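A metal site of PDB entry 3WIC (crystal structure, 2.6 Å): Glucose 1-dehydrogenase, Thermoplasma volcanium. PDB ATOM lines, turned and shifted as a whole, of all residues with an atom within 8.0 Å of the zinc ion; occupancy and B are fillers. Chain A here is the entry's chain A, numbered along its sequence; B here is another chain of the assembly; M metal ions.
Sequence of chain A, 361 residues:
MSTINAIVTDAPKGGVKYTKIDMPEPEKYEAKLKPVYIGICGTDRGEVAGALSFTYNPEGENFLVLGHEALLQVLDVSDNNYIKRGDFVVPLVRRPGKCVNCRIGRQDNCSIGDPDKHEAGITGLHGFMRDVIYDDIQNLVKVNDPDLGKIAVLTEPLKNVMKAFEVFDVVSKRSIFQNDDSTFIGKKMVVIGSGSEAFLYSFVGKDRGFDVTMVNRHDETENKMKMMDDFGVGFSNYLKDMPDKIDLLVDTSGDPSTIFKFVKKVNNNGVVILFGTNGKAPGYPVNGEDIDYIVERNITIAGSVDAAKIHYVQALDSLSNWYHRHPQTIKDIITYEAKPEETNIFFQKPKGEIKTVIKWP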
ATOM      1  N   ARG A  94      27.508  -2.504 -14.213  1.00  0.00           N
ATOM      2  CA  ARG A  94      26.307  -2.153 -14.995  1.00  0.00           C
ATOM      3  C   ARG A  94      26.486  -0.835 -15.689  1.00  0.00           C
ATOM      4  O   ARG A  94      26.924   0.127 -15.107  1.00  0.00           O
ATOM      5  CB  ARG A  94      25.090  -2.111 -14.115  1.00  0.00           C
ATOM      6  CG  ARG A  94      23.766  -2.018 -14.881  1.00  0.00           C
ATOM      7  CD  ARG A  94      22.615  -1.982 -13.879  1.00  0.00           C
ATOM      8  NE  ARG A  94      22.293  -3.321 -13.392  1.00  0.00           N
ATOM      9  CZ  ARG A  94      21.093  -3.733 -13.025  1.00  0.00           C
ATOM     10  NH1 ARG A  94      20.075  -2.892 -13.010  1.00  0.00           N
ATOM     11  NH2 ARG A  94      20.922  -4.996 -12.675  1.00  0.00           N
ATOM     12  N   ARG A  95      26.117  -0.847 -16.969  1.00  0.00           N
ATOM     13  CA  ARG A  95      26.180   0.289 -17.885  1.00  0.00           C
ATOM     14  C   ARG A  95      24.779   0.795 -18.167  1.00  0.00           C
ATOM     15  O   ARG A  95      23.856  -0.017 -18.332  1.00  0.00           O
ATOM     16  CB  ARG A  95      26.818  -0.169 -19.191  1.00  0.00           C
ATOM     17  CG  ARG A  95      28.153  -0.883 -19.006  1.00  0.00           C
ATOM     18  CD  ARG A  95      29.125   0.056 -18.340  1.00  0.00           C
ATOM     19  NE  ARG A  95      30.290  -0.532 -17.708  1.00  0.00           N
ATOM     20  CZ  ARG A  95      31.554  -0.267 -18.069  1.00  0.00           C
ATOM     21  NH1 ARG A  95      31.823   0.438 -19.173  1.00  0.00           N
ATOM     22  NH2 ARG A  95      32.546  -0.757 -17.362  1.00  0.00           N
ATOM     23  N   PRO A  96      24.623   2.132 -18.256  1.00  0.00           N
ATOM     24  CA  PRO A  96      23.309   2.706 -18.439  1.00  0.00           C
ATOM     25  C   PRO A  96      22.811   2.694 -19.899  1.00  0.00           C
ATOM     26  O   PRO A  96      23.588   2.983 -20.820  1.00  0.00           O
ATOM     27  CB  PRO A  96      23.522   4.155 -17.956  1.00  0.00           C
ATOM     28  CG  PRO A  96      24.904   4.470 -18.366  1.00  0.00           C
ATOM     29  CD  PRO A  96      25.667   3.185 -18.183  1.00  0.00           C
ATOM     30  N   GLY A  97      21.517   2.432 -20.085  1.00  0.00           N
ATOM     31  CA  GLY A  97      20.790   2.821 -21.295  1.00  0.00           C
ATOM     32  C   GLY A  97      20.063   4.150 -21.149  1.00  0.00           C
ATOM     33  O   GLY A  97      20.583   5.127 -20.549  1.00  0.00           O
ATOM     34  N   LYS A  98      18.840   4.177 -21.694  1.00  0.00           N
ATOM     35  CA  LYS A  98      18.121   5.424 -21.915  1.00  0.00           C
ATOM     36  C   LYS A  98      17.014   5.770 -20.883  1.00  0.00           C
ATOM     37  O   LYS A  98      16.437   6.867 -20.878  1.00  0.00           O
ATOM     38  CB  LYS A  98      17.541   5.392 -23.322  1.00  0.00           C
ATOM     39  CG  LYS A  98      18.545   5.124 -24.446  1.00  0.00           C
ATOM     40  CD  LYS A  98      19.684   6.140 -24.545  1.00  0.00           C
ATOM     41  CE  LYS A  98      19.193   7.503 -25.013  1.00  0.00           C
ATOM     42  NZ  LYS A  98      20.260   8.382 -25.592  1.00  0.00           N
ATOM     43  N   CYS A  99      16.714   4.825 -19.990  1.00  0.00           N
ATOM     44  CA  CYS A  99      15.489   4.980 -19.203  1.00  0.00           C
ATOM     45  C   CYS A  99      15.709   6.111 -18.225  1.00  0.00           C
ATOM     46  O   CYS A  99      16.813   6.589 -18.083  1.00  0.00           O
ATOM     47  CB  CYS A  99      15.104   3.668 -18.491  1.00  0.00           C
ATOM     48  SG  CYS A  99      15.892   3.436 -16.894  1.00  0.00           S
ATOM     49  N   VAL A 100      14.647   6.500 -17.527  1.00  0.00           N
ATOM     50  CA  VAL A 100      14.698   7.635 -16.614  1.00  0.00           C
ATOM     51  C   VAL A 100      15.680   7.439 -15.417  1.00  0.00           C
ATOM     52  O   VAL A 100      16.229   8.409 -14.882  1.00  0.00           O
ATOM     53  CB  VAL A 100      13.279   8.030 -16.178  1.00  0.00           C
ATOM     54  CG1 VAL A 100      12.611   6.953 -15.297  1.00  0.00           C
ATOM     55  CG2 VAL A 100      13.290   9.414 -15.489  1.00  0.00           C
ATOM     56  N   ASN A 101      15.898   6.185 -14.993  1.00  0.00           N
ATOM     57  CA  ASN A 101      16.936   5.892 -14.002  1.00  0.00           C
ATOM     58  C   ASN A 101      18.341   5.728 -14.601  1.00  0.00           C
ATOM     59  O   ASN A 101      19.328   6.174 -14.010  1.00  0.00           O
ATOM     60  CB  ASN A 101      16.566   4.653 -13.198  1.00  0.00           C
ATOM     61  CG  ASN A 101      15.506   4.949 -12.140  1.00  0.00           C
ATOM     62  OD1 ASN A 101      15.837   5.320 -11.026  1.00  0.00           O
ATOM     63  ND2 ASN A 101      14.245   4.797 -12.487  1.00  0.00           N
ATOM     64  N   CYS A 102      18.437   5.124 -15.783  1.00  0.00           N
ATOM     65  CA  CYS A 102      19.716   5.002 -16.434  1.00  0.00           C
ATOM     66  C   CYS A 102      20.313   6.372 -16.760  1.00  0.00           C
ATOM     67  O   CYS A 102      21.507   6.601 -16.558  1.00  0.00           O
ATOM     68  CB  CYS A 102      19.636   4.059 -17.660  1.00  0.00           C
ATOM     69  SG  CYS A 102      19.537   2.272 -17.203  1.00  0.00           S
ATOM     70  N   ARG A 103      19.516   7.337 -17.198  1.00  0.00           N
ATOM     71  CA  ARG A 103      20.147   8.612 -17.608  1.00  0.00           C
ATOM     72  C   ARG A 103      20.651   9.508 -16.456  1.00  0.00           C
ATOM     73  O   ARG A 103      21.351  10.469 -16.730  1.00  0.00           O
ATOM     74  CB  ARG A 103      19.261   9.407 -18.522  1.00  0.00           C
ATOM     75  CG  ARG A 103      18.044   9.964 -17.864  1.00  0.00           C
ATOM     76  CD  ARG A 103      16.905   9.413 -18.670  1.00  0.00           C
ATOM     77  NE  ARG A 103      16.137  10.399 -19.338  1.00  0.00           N
ATOM     78  CZ  ARG A 103      15.121  10.108 -20.130  1.00  0.00           C
ATOM     79  NH1 ARG A 103      14.792   8.846 -20.390  1.00  0.00           N
ATOM     80  NH2 ARG A 103      14.427  11.086 -20.672  1.00  0.00           N
ATOM     81  N   ARG A 106      21.707   5.800 -12.409  1.00  0.00           N
ATOM     82  CA  ARG A 106      21.115   4.833 -11.515  1.00  0.00           C
ATOM     83  C   ARG A 106      20.639   3.659 -12.329  1.00  0.00           C
ATOM     84  O   ARG A 106      19.525   3.132 -12.120  1.00  0.00           O
ATOM     85  CB  ARG A 106      19.951   5.430 -10.715  1.00  0.00           C
ATOM     86  CG  ARG A 106      20.344   6.496  -9.724  1.00  0.00           C
ATOM     87  CD  ARG A 106      21.336   6.019  -8.692  1.00  0.00           C
ATOM     88  NE  ARG A 106      20.885   4.881  -7.873  1.00  0.00           N
ATOM     89  CZ  ARG A 106      20.782   4.868  -6.538  1.00  0.00           C
ATOM     90  NH1 ARG A 106      21.029   5.941  -5.788  1.00  0.00           N
ATOM     91  NH2 ARG A 106      20.396   3.759  -5.950  1.00  0.00           N
ATOM     92  N   GLN A 107      21.518   3.236 -13.225  1.00  0.00           N
ATOM     93  CA  GLN A 107      21.266   2.059 -14.073  1.00  0.00           C
ATOM     94  C   GLN A 107      20.909   0.850 -13.190  1.00  0.00           C
ATOM     95  O   GLN A 107      20.158  -0.047 -13.642  1.00  0.00           O
ATOM     96  CB  GLN A 107      22.438   1.762 -15.036  1.00  0.00           C
ATOM     97  CG  GLN A 107      23.845   1.641 -14.440  1.00  0.00           C
ATOM     98  CD  GLN A 107      24.619   2.985 -14.331  1.00  0.00           C
ATOM     99  OE1 GLN A 107      24.023   4.065 -14.115  1.00  0.00           O
ATOM    100  NE2 GLN A 107      25.964   2.909 -14.470  1.00  0.00           N
ATOM    101  N   ASP A 108      21.417   0.909 -11.933  1.00  0.00           N
ATOM    102  CA  ASP A 108      21.100  -0.055 -10.859  1.00  0.00           C
ATOM    103  C   ASP A 108      19.631  -0.278 -10.669  1.00  0.00           C
ATOM    104  O   ASP A 108      19.224  -1.414 -10.489  1.00  0.00           O
ATOM    105  CB  ASP A 108      21.780   0.288  -9.522  1.00  0.00           C
ATOM    106  CG  ASP A 108      21.176   1.505  -8.799  1.00  0.00           C
ATOM    107  OD1 ASP A 108      21.277   2.634  -9.358  1.00  0.00           O
ATOM    108  OD2 ASP A 108      20.652   1.310  -7.671  1.00  0.00           O
ATOM    109  N   ASN A 109      18.870   0.795 -10.779  1.00  0.00           N
ATOM    110  CA  ASN A 109      17.405   0.773 -10.726  1.00  0.00           C
ATOM    111  C   ASN A 109      16.719   0.971 -12.043  1.00  0.00           C
ATOM    112  O   ASN A 109      15.697   1.638 -12.103  1.00  0.00           O
ATOM    113  CB  ASN A 109      16.938   1.848  -9.742  1.00  0.00           C
ATOM    114  CG  ASN A 109      17.424   1.565  -8.355  1.00  0.00           C
ATOM    115  OD1 ASN A 109      17.451   0.372  -7.928  1.00  0.00           O
ATOM    116  ND2 ASN A 109      17.848   2.621  -7.636  1.00  0.00           N
ATOM    117  N   CYS A 110      17.249   0.384 -13.102  1.00  0.00           N
ATOM    118  CA  CYS A 110      16.733   0.610 -14.442  1.00  0.00           C
ATOM    119  C   CYS A 110      15.290   0.219 -14.391  1.00  0.00           C
ATOM    120  O   CYS A 110      14.925  -0.760 -13.685  1.00  0.00           O
ATOM    121  CB  CYS A 110      17.475  -0.277 -15.460  1.00  0.00           C
ATOM    122  SG  CYS A 110      16.744  -0.372 -17.119  1.00  0.00           S
ATOM    123  N   SER A 111      14.447   0.950 -15.101  1.00  0.00           N
ATOM    124  CA  SER A 111      13.029   0.626 -15.032  1.00  0.00           C
ATOM    125  C   SER A 111      12.561  -0.288 -16.150  1.00  0.00           C
ATOM    126  O   SER A 111      11.392  -0.664 -16.161  1.00  0.00           O
ATOM    127  CB  SER A 111      12.151   1.886 -14.920  1.00  0.00           C
ATOM    128  OG  SER A 111      12.646   2.979 -15.607  1.00  0.00           O
ATOM    129  N   ILE A 112      13.490  -0.656 -17.039  1.00  0.00           N
ATOM    130  CA  ILE A 112      13.182  -1.498 -18.190  1.00  0.00           C
ATOM    131  C   ILE A 112      13.772  -2.893 -18.078  1.00  0.00           C
ATOM    132  O   ILE A 112      13.101  -3.856 -18.411  1.00  0.00           O
ATOM    133  CB  ILE A 112      13.601  -0.799 -19.507  1.00  0.00           C
ATOM    134  CG1 ILE A 112      12.723   0.447 -19.719  1.00  0.00           C
ATOM    135  CG2 ILE A 112      13.491  -1.742 -20.692  1.00  0.00           C
ATOM    136  CD1 ILE A 112      13.201   1.369 -20.795  1.00  0.00           C
ATOM    137  N   GLY A 113      15.008  -3.012 -17.594  1.00  0.00           N
ATOM    138  CA  GLY A 113      15.742  -4.286 -17.611  1.00  0.00           C
ATOM    139  C   GLY A 113      16.473  -4.500 -18.921  1.00  0.00           C
ATOM    140  O   GLY A 113      16.642  -3.528 -19.687  1.00  0.00           O
ATOM    141  N   ASP A 114      16.918  -5.722 -19.192  1.00  0.00           N
ATOM    142  CA  ASP A 114      17.494  -6.004 -20.522  1.00  0.00           C
ATOM    143  C   ASP A 114      16.425  -5.666 -21.579  1.00  0.00           C
ATOM    144  O   ASP A 114      15.259  -6.049 -21.402  1.00  0.00           O
ATOM    145  CB  ASP A 114      18.012  -7.448 -20.660  1.00  0.00           C
ATOM    146  CG  ASP A 114      19.100  -7.797 -19.602  1.00  0.00           C
ATOM    147  OD1 ASP A 114      20.165  -7.097 -19.471  1.00  0.00           O
ATOM    148  OD2 ASP A 114      18.890  -8.815 -18.886  1.00  0.00           O
ATOM    149  N   PRO A 115      16.818  -4.974 -22.666  1.00  0.00           N
ATOM    150  CA  PRO A 115      18.221  -4.723 -22.973  1.00  0.00           C
ATOM    151  C   PRO A 115      18.615  -3.242 -22.858  1.00  0.00           C
ATOM    152  O   PRO A 115      19.413  -2.764 -23.638  1.00  0.00           O
ATOM    153  CB  PRO A 115      18.269  -5.137 -24.453  1.00  0.00           C
ATOM    154  CG  PRO A 115      16.991  -4.518 -24.974  1.00  0.00           C
ATOM    155  CD  PRO A 115      15.994  -4.537 -23.814  1.00  0.00           C
ATOM    156  N   ASP A 116      18.022  -2.521 -21.934  1.00  0.00           N
ATOM    157  CA  ASP A 116      18.325  -1.125 -21.817  1.00  0.00           C
ATOM    158  C   ASP A 116      19.588  -0.939 -20.993  1.00  0.00           C
ATOM    159  O   ASP A 116      20.265   0.047 -21.109  1.00  0.00           O
ATOM    160  CB  ASP A 116      17.190  -0.379 -21.130  1.00  0.00           C
ATOM    161  CG  ASP A 116      17.310   1.131 -21.283  1.00  0.00           C
ATOM    162  OD1 ASP A 116      17.689   1.572 -22.401  1.00  0.00           O
ATOM    163  OD2 ASP A 116      17.071   1.852 -20.284  1.00  0.00           O
ATOM    164  N   LYS A 117      19.882  -1.894 -20.145  1.00  0.00           N
ATOM    165  CA  LYS A 117      21.053  -1.850 -19.312  1.00  0.00           C
ATOM    166  C   LYS A 117      21.871  -3.114 -19.613  1.00  0.00           C
ATOM    167  O   LYS A 117      21.340  -4.081 -20.163  1.00  0.00           O
ATOM    168  CB  LYS A 117      20.609  -1.699 -17.849  1.00  0.00           C
ATOM    169  CG  LYS A 117      20.789  -2.882 -16.923  1.00  0.00           C
ATOM    170  CD  LYS A 117      19.825  -4.025 -17.106  1.00  0.00           C
ATOM    171  CE  LYS A 117      20.167  -5.147 -16.102  1.00  0.00           C
ATOM    172  NZ  LYS A 117      19.867  -6.521 -16.538  1.00  0.00           N
ATOM    173  N   HIS A 118      23.145  -3.085 -19.238  1.00  0.00           N
ATOM    174  CA  HIS A 118      24.067  -4.187 -19.519  1.00  0.00           C
ATOM    175  C   HIS A 118      25.124  -4.277 -18.403  1.00  0.00           C
ATOM    176  O   HIS A 118      25.632  -3.231 -17.925  1.00  0.00           O
ATOM    177  CB  HIS A 118      24.756  -3.995 -20.893  1.00  0.00           C
ATOM    178  CG  HIS A 118      23.807  -4.033 -22.048  1.00  0.00           C
ATOM    179  ND1 HIS A 118      23.263  -2.901 -22.599  1.00  0.00           N
ATOM    180  CD2 HIS A 118      23.316  -5.070 -22.760  1.00  0.00           C
ATOM    181  CE1 HIS A 118      22.451  -3.235 -23.591  1.00  0.00           C
ATOM    182  NE2 HIS A 118      22.470  -4.542 -23.704  1.00  0.00           N
ATOM    183  N   ASN B 269      11.129  -1.877 -10.353  1.00  0.00           N
ATOM    184  CA  ASN B 269      10.770  -0.856  -9.355  1.00  0.00           C
ATOM    185  C   ASN B 269       9.303  -0.842  -8.989  1.00  0.00           C
ATOM    186  O   ASN B 269       8.791   0.121  -8.461  1.00  0.00           O
ATOM    187  CB  ASN B 269      11.229   0.548  -9.806  1.00  0.00           C
ATOM    188  CG  ASN B 269      12.650   0.536 -10.316  1.00  0.00           C
ATOM    189  OD1 ASN B 269      12.935   0.893 -11.449  1.00  0.00           O
ATOM    190  ND2 ASN B 269      13.546   0.117  -9.495  1.00  0.00           N
HETATM  191 ZN    ZN M   1      17.471   1.713 -17.866  1.00  0.00          ZN
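N of Ser 111 lies close to SG of Cys 99, at 3.4 Å.
The side-chain sulfur of Cys 102 lies close to the backbone NH of Gly 97 (3.5 Å).
The side-chain sulfur (SG) of Cys 110 sits close to the backbone NH (N) of Ile 112, 3.3 Å away.
N of Gly 113 lies close to SG of Cys 110 (3.2 Å).
The side-chain carboxylate (OD1) of Asp 116 sits at hydrogen-bond distance from the backbone NH (N) of Lys 98 (2.9 Å).
The backbone carbonyl oxygen of Asp 116 sits close to the backbone NH of Gly 97, 2.9 Å away.
The backbone carbonyl oxygen (O) of Cys 110 sits close to the side-chain amide oxygen (OD1) of Asn 269 of chain B, at 3.4 Å.
The side-chain sulfur (SG) of Cys 99 lies close to the backbone NH (N) of Asn 101 (3.3 Å).
Four residues have an atom within 4 Å of the zinc ion: Cys 99, Cys 102, Cys 110 and Asp 116.
The nearest printed residue that does not touch the zinc ion is Ser 111 (4.2 Å).
The side-chain sulfur (SG) of Cys 102 is bound to the zinc ion (2.2 Å).
SG of Cys 110 is bound to the zinc ion (2.3 Å).
The zinc ion is bound by OD2 of Asp 116, 2.5 Å away.
The zinc ion is bound by SG of Cys 99, 2.5 Å away.
The zinc ion has four donor atoms within binding distance.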
